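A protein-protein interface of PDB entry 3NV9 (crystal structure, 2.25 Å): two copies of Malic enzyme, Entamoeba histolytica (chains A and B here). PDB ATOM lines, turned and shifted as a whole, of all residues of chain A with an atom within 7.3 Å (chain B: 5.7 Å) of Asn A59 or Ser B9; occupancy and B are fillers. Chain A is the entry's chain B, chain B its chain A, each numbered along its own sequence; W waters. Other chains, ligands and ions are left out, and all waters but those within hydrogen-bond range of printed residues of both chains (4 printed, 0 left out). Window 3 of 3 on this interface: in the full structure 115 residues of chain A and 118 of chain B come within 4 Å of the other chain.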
ATOM      1  N   ALA A  56       4.908  23.774  10.488  1.00  0.00           N
ATOM      2  CA  ALA A  56       3.801  24.400  11.216  1.00  0.00           C
ATOM      3  C   ALA A  56       2.421  23.905  10.840  1.00  0.00           C
ATOM      4  O   ALA A  56       1.482  24.051  11.617  1.00  0.00           O
ATOM      5  CB  ALA A  56       3.845  25.963  11.062  1.00  0.00           C
ATOM      6  N   GLY A  57       2.284  23.335   9.655  1.00  0.00           N
ATOM      7  CA  GLY A  57       0.987  22.910   9.190  1.00  0.00           C
ATOM      8  C   GLY A  57       1.045  22.319   7.808  1.00  0.00           C
ATOM      9  O   GLY A  57       2.025  22.506   7.058  1.00  0.00           O
ATOM     10  N   PHE A  58      -0.051  21.655   7.449  1.00  0.00           N
ATOM     11  CA  PHE A  58      -0.104  20.838   6.254  1.00  0.00           C
ATOM     12  C   PHE A  58       0.320  21.602   5.008  1.00  0.00           C
ATOM     13  O   PHE A  58       1.051  21.092   4.190  1.00  0.00           O
ATOM     14  CB  PHE A  58      -1.501  20.240   6.056  1.00  0.00           C
ATOM     15  CG  PHE A  58      -1.709  19.679   4.676  1.00  0.00           C
ATOM     16  CD1 PHE A  58      -1.285  18.387   4.374  1.00  0.00           C
ATOM     17  CD2 PHE A  58      -2.280  20.445   3.681  1.00  0.00           C
ATOM     18  CE1 PHE A  58      -1.433  17.841   3.077  1.00  0.00           C
ATOM     19  CE2 PHE A  58      -2.443  19.942   2.395  1.00  0.00           C
ATOM     20  CZ  PHE A  58      -2.011  18.644   2.071  1.00  0.00           C
ATOM     21  N   ASN A  59      -0.128  22.833   4.871  1.00  0.00           N
ATOM     22  CA  ASN A  59       0.090  23.554   3.650  1.00  0.00           C
ATOM     23  C   ASN A  59       1.556  23.978   3.375  1.00  0.00           C
ATOM     24  O   ASN A  59       1.886  24.370   2.267  1.00  0.00           O
ATOM     25  CB  ASN A  59      -0.855  24.738   3.607  1.00  0.00           C
ATOM     26  CG  ASN A  59      -2.340  24.307   3.455  1.00  0.00           C
ATOM     27  OD1 ASN A  59      -3.107  24.220   4.437  1.00  0.00           O
ATOM     28  ND2 ASN A  59      -2.721  24.023   2.249  1.00  0.00           N
ATOM     29  N   TRP A  60       2.431  23.876   4.375  1.00  0.00           N
ATOM     30  CA  TRP A  60       3.853  24.138   4.146  1.00  0.00           C
ATOM     31  C   TRP A  60       4.435  23.128   3.085  1.00  0.00           C
ATOM     32  O   TRP A  60       5.439  23.417   2.355  1.00  0.00           O
ATOM     33  CB  TRP A  60       4.610  24.097   5.481  1.00  0.00           C
ATOM     34  CG  TRP A  60       4.555  25.453   6.171  1.00  0.00           C
ATOM     35  CD1 TRP A  60       3.721  25.840   7.208  1.00  0.00           C
ATOM     36  CD2 TRP A  60       5.323  26.602   5.828  1.00  0.00           C
ATOM     37  NE1 TRP A  60       3.937  27.143   7.523  1.00  0.00           N
ATOM     38  CE2 TRP A  60       4.929  27.640   6.713  1.00  0.00           C
ATOM     39  CE3 TRP A  60       6.322  26.851   4.875  1.00  0.00           C
ATOM     40  CZ2 TRP A  60       5.483  28.933   6.659  1.00  0.00           C
ATOM     41  CZ3 TRP A  60       6.888  28.133   4.821  1.00  0.00           C
ATOM     42  CH2 TRP A  60       6.444  29.168   5.701  1.00  0.00           C
ATOM     43  N   PHE A  61       3.819  21.943   3.033  1.00  0.00           N
ATOM     44  CA  PHE A  61       4.193  20.986   2.025  1.00  0.00           C
ATOM     45  C   PHE A  61       4.010  21.547   0.594  1.00  0.00           C
ATOM     46  O   PHE A  61       4.738  21.162  -0.295  1.00  0.00           O
ATOM     47  CB  PHE A  61       3.367  19.712   2.156  1.00  0.00           C
ATOM     48  CG  PHE A  61       3.653  18.929   3.376  1.00  0.00           C
ATOM     49  CD1 PHE A  61       4.960  18.754   3.812  1.00  0.00           C
ATOM     50  CD2 PHE A  61       2.600  18.343   4.100  1.00  0.00           C
ATOM     51  CE1 PHE A  61       5.240  18.004   4.961  1.00  0.00           C
ATOM     52  CE2 PHE A  61       2.854  17.603   5.242  1.00  0.00           C
ATOM     53  CZ  PHE A  61       4.176  17.419   5.675  1.00  0.00           C
ATOM     54  N   ASN A  62       3.010  22.402   0.372  1.00  0.00           N
ATOM     55  CA  ASN A  62       2.811  23.040  -0.944  1.00  0.00           C
ATOM     56  C   ASN A  62       3.986  23.899  -1.401  1.00  0.00           C
ATOM     57  O   ASN A  62       4.079  24.237  -2.601  1.00  0.00           O
ATOM     58  CB  ASN A  62       1.529  23.858  -0.931  1.00  0.00           C
ATOM     59  CG  ASN A  62       0.297  22.967  -0.653  1.00  0.00           C
ATOM     60  OD1 ASN A  62       0.322  21.795  -0.999  1.00  0.00           O
ATOM     61  ND2 ASN A  62      -0.715  23.495   0.070  1.00  0.00           N
ATOM     62  N   ALA A  63       4.852  24.274  -0.441  1.00  0.00           N
ATOM     63  CA  ALA A  63       6.027  25.105  -0.708  1.00  0.00           C
ATOM     64  C   ALA A  63       7.276  24.193  -0.728  1.00  0.00           C
ATOM     65  O   ALA A  63       8.200  24.423  -1.507  1.00  0.00           O
ATOM     66  CB  ALA A  63       6.175  26.198   0.324  1.00  0.00           C
ATOM     67  N   TYR A  64       7.268  23.141   0.082  1.00  0.00           N
ATOM     68  CA  TYR A  64       8.334  22.155   0.093  1.00  0.00           C
ATOM     69  C   TYR A  64       8.303  21.123  -1.046  1.00  0.00           C
ATOM     70  O   TYR A  64       9.312  20.431  -1.322  1.00  0.00           O
ATOM     71  CB  TYR A  64       8.340  21.405   1.439  1.00  0.00           C
ATOM     72  CG  TYR A  64       8.629  22.265   2.627  1.00  0.00           C
ATOM     73  CD1 TYR A  64       9.514  23.336   2.543  1.00  0.00           C
ATOM     74  CD2 TYR A  64       7.991  22.018   3.860  1.00  0.00           C
ATOM     75  CE1 TYR A  64       9.753  24.154   3.660  1.00  0.00           C
ATOM     76  CE2 TYR A  64       8.241  22.814   4.968  1.00  0.00           C
ATOM     77  CZ  TYR A  64       9.130  23.882   4.868  1.00  0.00           C
ATOM     78  OH  TYR A  64       9.393  24.675   5.999  1.00  0.00           O
ATOM     79  N   THR A  66       5.086  19.922  -4.360  1.00  0.00           N
ATOM     80  CA  THR A  66       4.289  20.530  -5.426  1.00  0.00           C
ATOM     81  C   THR A  66       3.148  21.309  -4.830  1.00  0.00           C
ATOM     82  O   THR A  66       2.564  20.854  -3.851  1.00  0.00           O
ATOM     83  CB  THR A  66       3.656  19.486  -6.355  1.00  0.00           C
ATOM     84  OG1 THR A  66       3.072  18.432  -5.549  1.00  0.00           O
ATOM     85  CG2 THR A  66       4.661  18.909  -7.176  1.00  0.00           C
ATOM     86  N   PRO A  67       2.813  22.472  -5.426  1.00  0.00           N
ATOM     87  CA  PRO A  67       3.460  22.974  -6.658  1.00  0.00           C
ATOM     88  C   PRO A  67       4.707  23.797  -6.409  1.00  0.00           C
ATOM     89  O   PRO A  67       5.492  23.962  -7.336  1.00  0.00           O
ATOM     90  CB  PRO A  67       2.381  23.892  -7.270  1.00  0.00           C
ATOM     91  CG  PRO A  67       1.702  24.526  -6.006  1.00  0.00           C
ATOM     92  CD  PRO A  67       1.743  23.370  -4.934  1.00  0.00           C
ATOM     93  N   LYS B   5      -1.949  32.923   8.527  1.00  0.00           N
ATOM     94  CA  LYS B   5      -1.553  32.267   9.780  1.00  0.00           C
ATOM     95  C   LYS B   5      -0.224  31.561   9.653  1.00  0.00           C
ATOM     96  O   LYS B   5       0.119  31.070   8.572  1.00  0.00           O
ATOM     97  CB  LYS B   5      -2.600  31.238  10.222  1.00  0.00           C
ATOM     98  CG  LYS B   5      -3.962  31.862  10.508  1.00  0.00           C
ATOM     99  CD  LYS B   5      -4.907  30.879  11.110  1.00  0.00           C
ATOM    100  CE  LYS B   5      -6.247  31.555  11.255  1.00  0.00           C
ATOM    101  NZ  LYS B   5      -7.213  30.573  11.792  1.00  0.00           N
ATOM    102  N   ASP B   7       0.529  28.706  10.250  1.00  0.00           N
ATOM    103  CA  ASP B   7       0.383  27.325   9.782  1.00  0.00           C
ATOM    104  C   ASP B   7      -0.109  27.243   8.361  1.00  0.00           C
ATOM    105  O   ASP B   7      -0.318  26.141   7.843  1.00  0.00           O
ATOM    106  CB  ASP B   7      -0.472  26.469  10.750  1.00  0.00           C
ATOM    107  CG  ASP B   7      -1.962  26.828  10.729  1.00  0.00           C
ATOM    108  OD1 ASP B   7      -2.404  27.803  10.046  1.00  0.00           O
ATOM    109  OD2 ASP B   7      -2.700  26.097  11.414  1.00  0.00           O
ATOM    110  N   LEU B   8      -0.315  28.401   7.744  1.00  0.00           N
ATOM    111  CA  LEU B   8      -0.740  28.465   6.331  1.00  0.00           C
ATOM    112  C   LEU B   8      -2.141  27.876   6.018  1.00  0.00           C
ATOM    113  O   LEU B   8      -2.426  27.581   4.855  1.00  0.00           O
ATOM    114  CB  LEU B   8       0.291  27.776   5.428  1.00  0.00           C
ATOM    115  CG  LEU B   8       1.454  28.705   5.134  1.00  0.00           C
ATOM    116  CD1 LEU B   8       2.463  27.973   4.159  1.00  0.00           C
ATOM    117  CD2 LEU B   8       0.974  30.080   4.598  1.00  0.00           C
ATOM    118  N   SER B   9      -2.960  27.672   7.051  1.00  0.00           N
ATOM    119  CA  SER B   9      -4.329  27.076   6.921  1.00  0.00           C
ATOM    120  C   SER B   9      -5.396  27.965   6.269  1.00  0.00           C
ATOM    121  O   SER B   9      -6.448  27.473   5.878  1.00  0.00           O
ATOM    122  CB  SER B   9      -4.858  26.611   8.302  1.00  0.00           C
ATOM    123  OG  SER B   9      -4.576  27.616   9.292  1.00  0.00           O
ATOM    124  N   ASN B  10      -5.142  29.264   6.144  1.00  0.00           N
ATOM    125  CA  ASN B  10      -6.185  30.194   5.776  1.00  0.00           C
ATOM    126  C   ASN B  10      -5.826  30.992   4.531  1.00  0.00           C
ATOM    127  O   ASN B  10      -6.181  32.171   4.412  1.00  0.00           O
ATOM    128  CB  ASN B  10      -6.474  31.148   6.939  1.00  0.00           C
ATOM    129  CG  ASN B  10      -5.296  32.098   7.243  1.00  0.00           C
ATOM    130  OD1 ASN B  10      -4.109  31.750   7.064  1.00  0.00           O
ATOM    131  ND2 ASN B  10      -5.626  33.304   7.734  1.00  0.00           N
ATOM    132  N   LEU B  11      -5.111  30.357   3.611  1.00  0.00           N
ATOM    133  CA  LEU B  11      -4.695  31.059   2.408  1.00  0.00           C
ATOM    134  C   LEU B  11      -5.911  31.494   1.575  1.00  0.00           C
ATOM    135  O   LEU B  11      -5.940  32.622   1.114  1.00  0.00           O
ATOM    136  CB  LEU B  11      -3.714  30.243   1.562  1.00  0.00           C
ATOM    137  CG  LEU B  11      -3.448  30.850   0.174  1.00  0.00           C
ATOM    138  CD1 LEU B  11      -2.563  32.067   0.221  1.00  0.00           C
ATOM    139  CD2 LEU B  11      -2.840  29.803  -0.756  1.00  0.00           C
ATOM    140  N   GLU B  12      -6.878  30.593   1.397  1.00  0.00           N
ATOM    141  CA  GLU B  12      -8.124  30.874   0.690  1.00  0.00           C
ATOM    142  C   GLU B  12      -8.756  32.215   1.095  1.00  0.00           C
ATOM    143  O   GLU B  12      -9.127  33.024   0.226  1.00  0.00           O
ATOM    144  CB  GLU B  12      -9.137  29.720   0.835  1.00  0.00           C
ATOM    145  CG  GLU B  12      -8.656  28.346   0.281  1.00  0.00           C
ATOM    146  CD  GLU B  12      -8.503  28.260  -1.258  1.00  0.00           C
ATOM    147  OE1 GLU B  12      -9.251  28.938  -2.008  1.00  0.00           O
ATOM    148  OE2 GLU B  12      -7.635  27.472  -1.722  1.00  0.00           O
ATOM    149  N   GLU B  13      -8.806  32.468   2.391  1.00  0.00           N
ATOM    150  CA  GLU B  13      -9.435  33.675   2.950  1.00  0.00           C
ATOM    151  C   GLU B  13      -8.554  34.905   2.798  1.00  0.00           C
ATOM    152  O   GLU B  13      -9.037  36.023   2.868  1.00  0.00           O
ATOM    153  CB  GLU B  13      -9.783  33.455   4.429  1.00  0.00           C
ATOM    154  CG  GLU B  13     -10.750  32.270   4.677  1.00  0.00           C
ATOM    155  CD  GLU B  13     -10.075  30.846   4.747  1.00  0.00           C
ATOM    156  OE1 GLU B  13      -9.026  30.565   4.123  1.00  0.00           O
ATOM    157  OE2 GLU B  13     -10.621  29.966   5.435  1.00  0.00           O
ATOM    158  N   TYR B  32       2.801  29.890  -3.755  1.00  0.00           N
ATOM    159  CA  TYR B  32       3.586  28.744  -3.368  1.00  0.00           C
ATOM    160  C   TYR B  32       4.922  28.666  -4.056  1.00  0.00           C
ATOM    161  O   TYR B  32       5.899  28.293  -3.418  1.00  0.00           O
ATOM    162  CB  TYR B  32       2.814  27.450  -3.494  1.00  0.00           C
ATOM    163  CG  TYR B  32       1.800  27.286  -2.375  1.00  0.00           C
ATOM    164  CD1 TYR B  32       2.203  27.246  -1.030  1.00  0.00           C
ATOM    165  CD2 TYR B  32       0.444  27.187  -2.651  1.00  0.00           C
ATOM    166  CE1 TYR B  32       1.286  27.123  -0.021  1.00  0.00           C
ATOM    167  CE2 TYR B  32      -0.478  27.058  -1.631  1.00  0.00           C
ATOM    168  CZ  TYR B  32      -0.059  27.019  -0.342  1.00  0.00           C
ATOM    169  OH  TYR B  32      -1.002  26.881   0.646  1.00  0.00           O
ATOM    170  N   GLY B 351      -1.345  19.775  -3.106  1.00  0.00           N
ATOM    171  CA  GLY B 351      -2.043  19.876  -1.816  1.00  0.00           C
ATOM    172  C   GLY B 351      -2.808  21.159  -1.576  1.00  0.00           C
ATOM    173  O   GLY B 351      -3.348  21.365  -0.492  1.00  0.00           O
ATOM    174  N   ASP B 352      -2.846  22.059  -2.573  1.00  0.00           N
ATOM    175  CA  ASP B 352      -3.616  23.276  -2.411  1.00  0.00           C
ATOM    176  C   ASP B 352      -4.982  23.220  -3.079  1.00  0.00           C
ATOM    177  O   ASP B 352      -5.740  24.234  -3.061  1.00  0.00           O
ATOM    178  CB  ASP B 352      -2.823  24.532  -2.786  1.00  0.00           C
ATOM    179  CG  ASP B 352      -2.395  24.554  -4.249  1.00  0.00           C
ATOM    180  OD1 ASP B 352      -1.990  23.532  -4.843  1.00  0.00           O
ATOM    181  OD2 ASP B 352      -2.408  25.660  -4.792  1.00  0.00           O
HETATM  182  O   HOH W   1      -4.985  23.174   0.886  1.00  0.00           O
HETATM  183  O   HOH W   2      -3.435  26.297   0.616  1.00  0.00           O
HETATM  184  O   HOH W   3      -1.803  24.149   6.652  1.00  0.00           O
HETATM  185  O   HOH W   4       1.752  19.300  -1.781  1.00  0.00           O
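The backbone carbonyl oxygen of Leu B8 lies close to the side-chain amide oxygen of Asn A59 (3.5 Å). The side-chain amide nitrogen (ND2) of Asn A62 sits at hydrogen-bond distance from the side-chain hydroxyl (OH) of Tyr B32 (3.4 Å). N of Gly B351 lies close to OD1 of Asn A62, 3.4 Å away.
The side-chain carboxylate of Asp B7 sits at hydrogen-bond distance from the backbone NH of Ser B9, 3.0 Å away. ND2 of Asn A62 lies close to ND2 of Asn A59, at 3.0 Å.
CB of Asp B7 touches O of Ala A56 (3.2 Å). Gly A57 touches Asp B7. Phe A58 touches Gly B351. Ser B9 touches Asn A59 (CA to OD1, 3.98 Å). Tyr B32 touches Asn A59. Asn A59 touches Gly B351. Leu B8 touches Trp A60 (CD1 to CE2, 3.6 Å). Asn A62 touches Asp B352. CD of Pro A67 touches OD1 of Asp B352, 3.7 Å away.
Printed residues of chain B within 4 Å of Ala A56: Asp B7 (3.2 Å). Printed residues of chain B within 4 Å of Gly A57: Asp B7. Of chain B, only Leu B8, Ser B9, Tyr B32 and Gly B351 come within 4 Å of Asn A59. Lys B5 touches none of the printed residues of chain A. Printed residues of chain A within 4 Å of Leu B8: Asn A59 (3.5 Å) and Trp A60 (3.6 Å). Of chain A, only Asn A59 (3.98 Å) comes within 4 Å of Ser B9. Asn B10 touches none of the printed residues of chain A. The nearest residue of chain B that does not touch Asn A59 is Asp B7 (4.5 Å). The nearest residue of chain A that does not touch Ser B9 is Gly A57 (6.5 Å). The nearest printed residue of chain A that does not touch Asp B7 is Trp A60 (4.1 Å).
Of the 11 printed residues of chain A, 7 touch a printed residue of chain B. Printed residues of chain A that touch a printed residue of chain B: Ala A56, Gly A57, Phe A58, Asn A59, Trp A60, Asn A62 and Pro A67. Hydrophobic or aromatic side chains of chain A that line the printed part of chain B: Ala A56, Phe A58, Trp A60 and Pro A67. Printed residues of chain B that touch a printed residue of chain A: Asp B7, Leu B8, Ser B9, Tyr B32, Gly B351 and Asp B352. Hydrophobic or aromatic side chains of chain B that line the printed part of chain A: Leu B8 and Tyr B32. Among the printed residues, 12 pairs touch across the chains. Among the printed residues, no Asp or Glu carboxylate lies within 4 Å of a Lys or Arg side-chain nitrogen of the other chain.
No position is printed for both chains.
Water W2 bridges OH of Tyr B32 (2.5 Å) and ND2 of Asn A59 (2.9 Å). Water W3 lies within hydrogen-bond range of the side-chain amide oxygen (OD1) of Asn A59 (2.6 Å), the backbone carbonyl oxygen (O) of Asp B7 (2.8 Å) and the backbone NH (N) of Phe A58 (3.2 Å). Water W4 lies within hydrogen-bond range of the backbone carbonyl oxygen of Thr A66 (2.7 Å), the side-chain amide oxygen of Asn A62 (3.0 Å) and the backbone NH of Gly B351 (3.4 Å). Water W1 lies within hydrogen-bond range of the side-chain amide nitrogen (ND2) of Asn A59 (2.8 Å) and the backbone carbonyl oxygen (O) of Gly B351 (2.8 Å).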
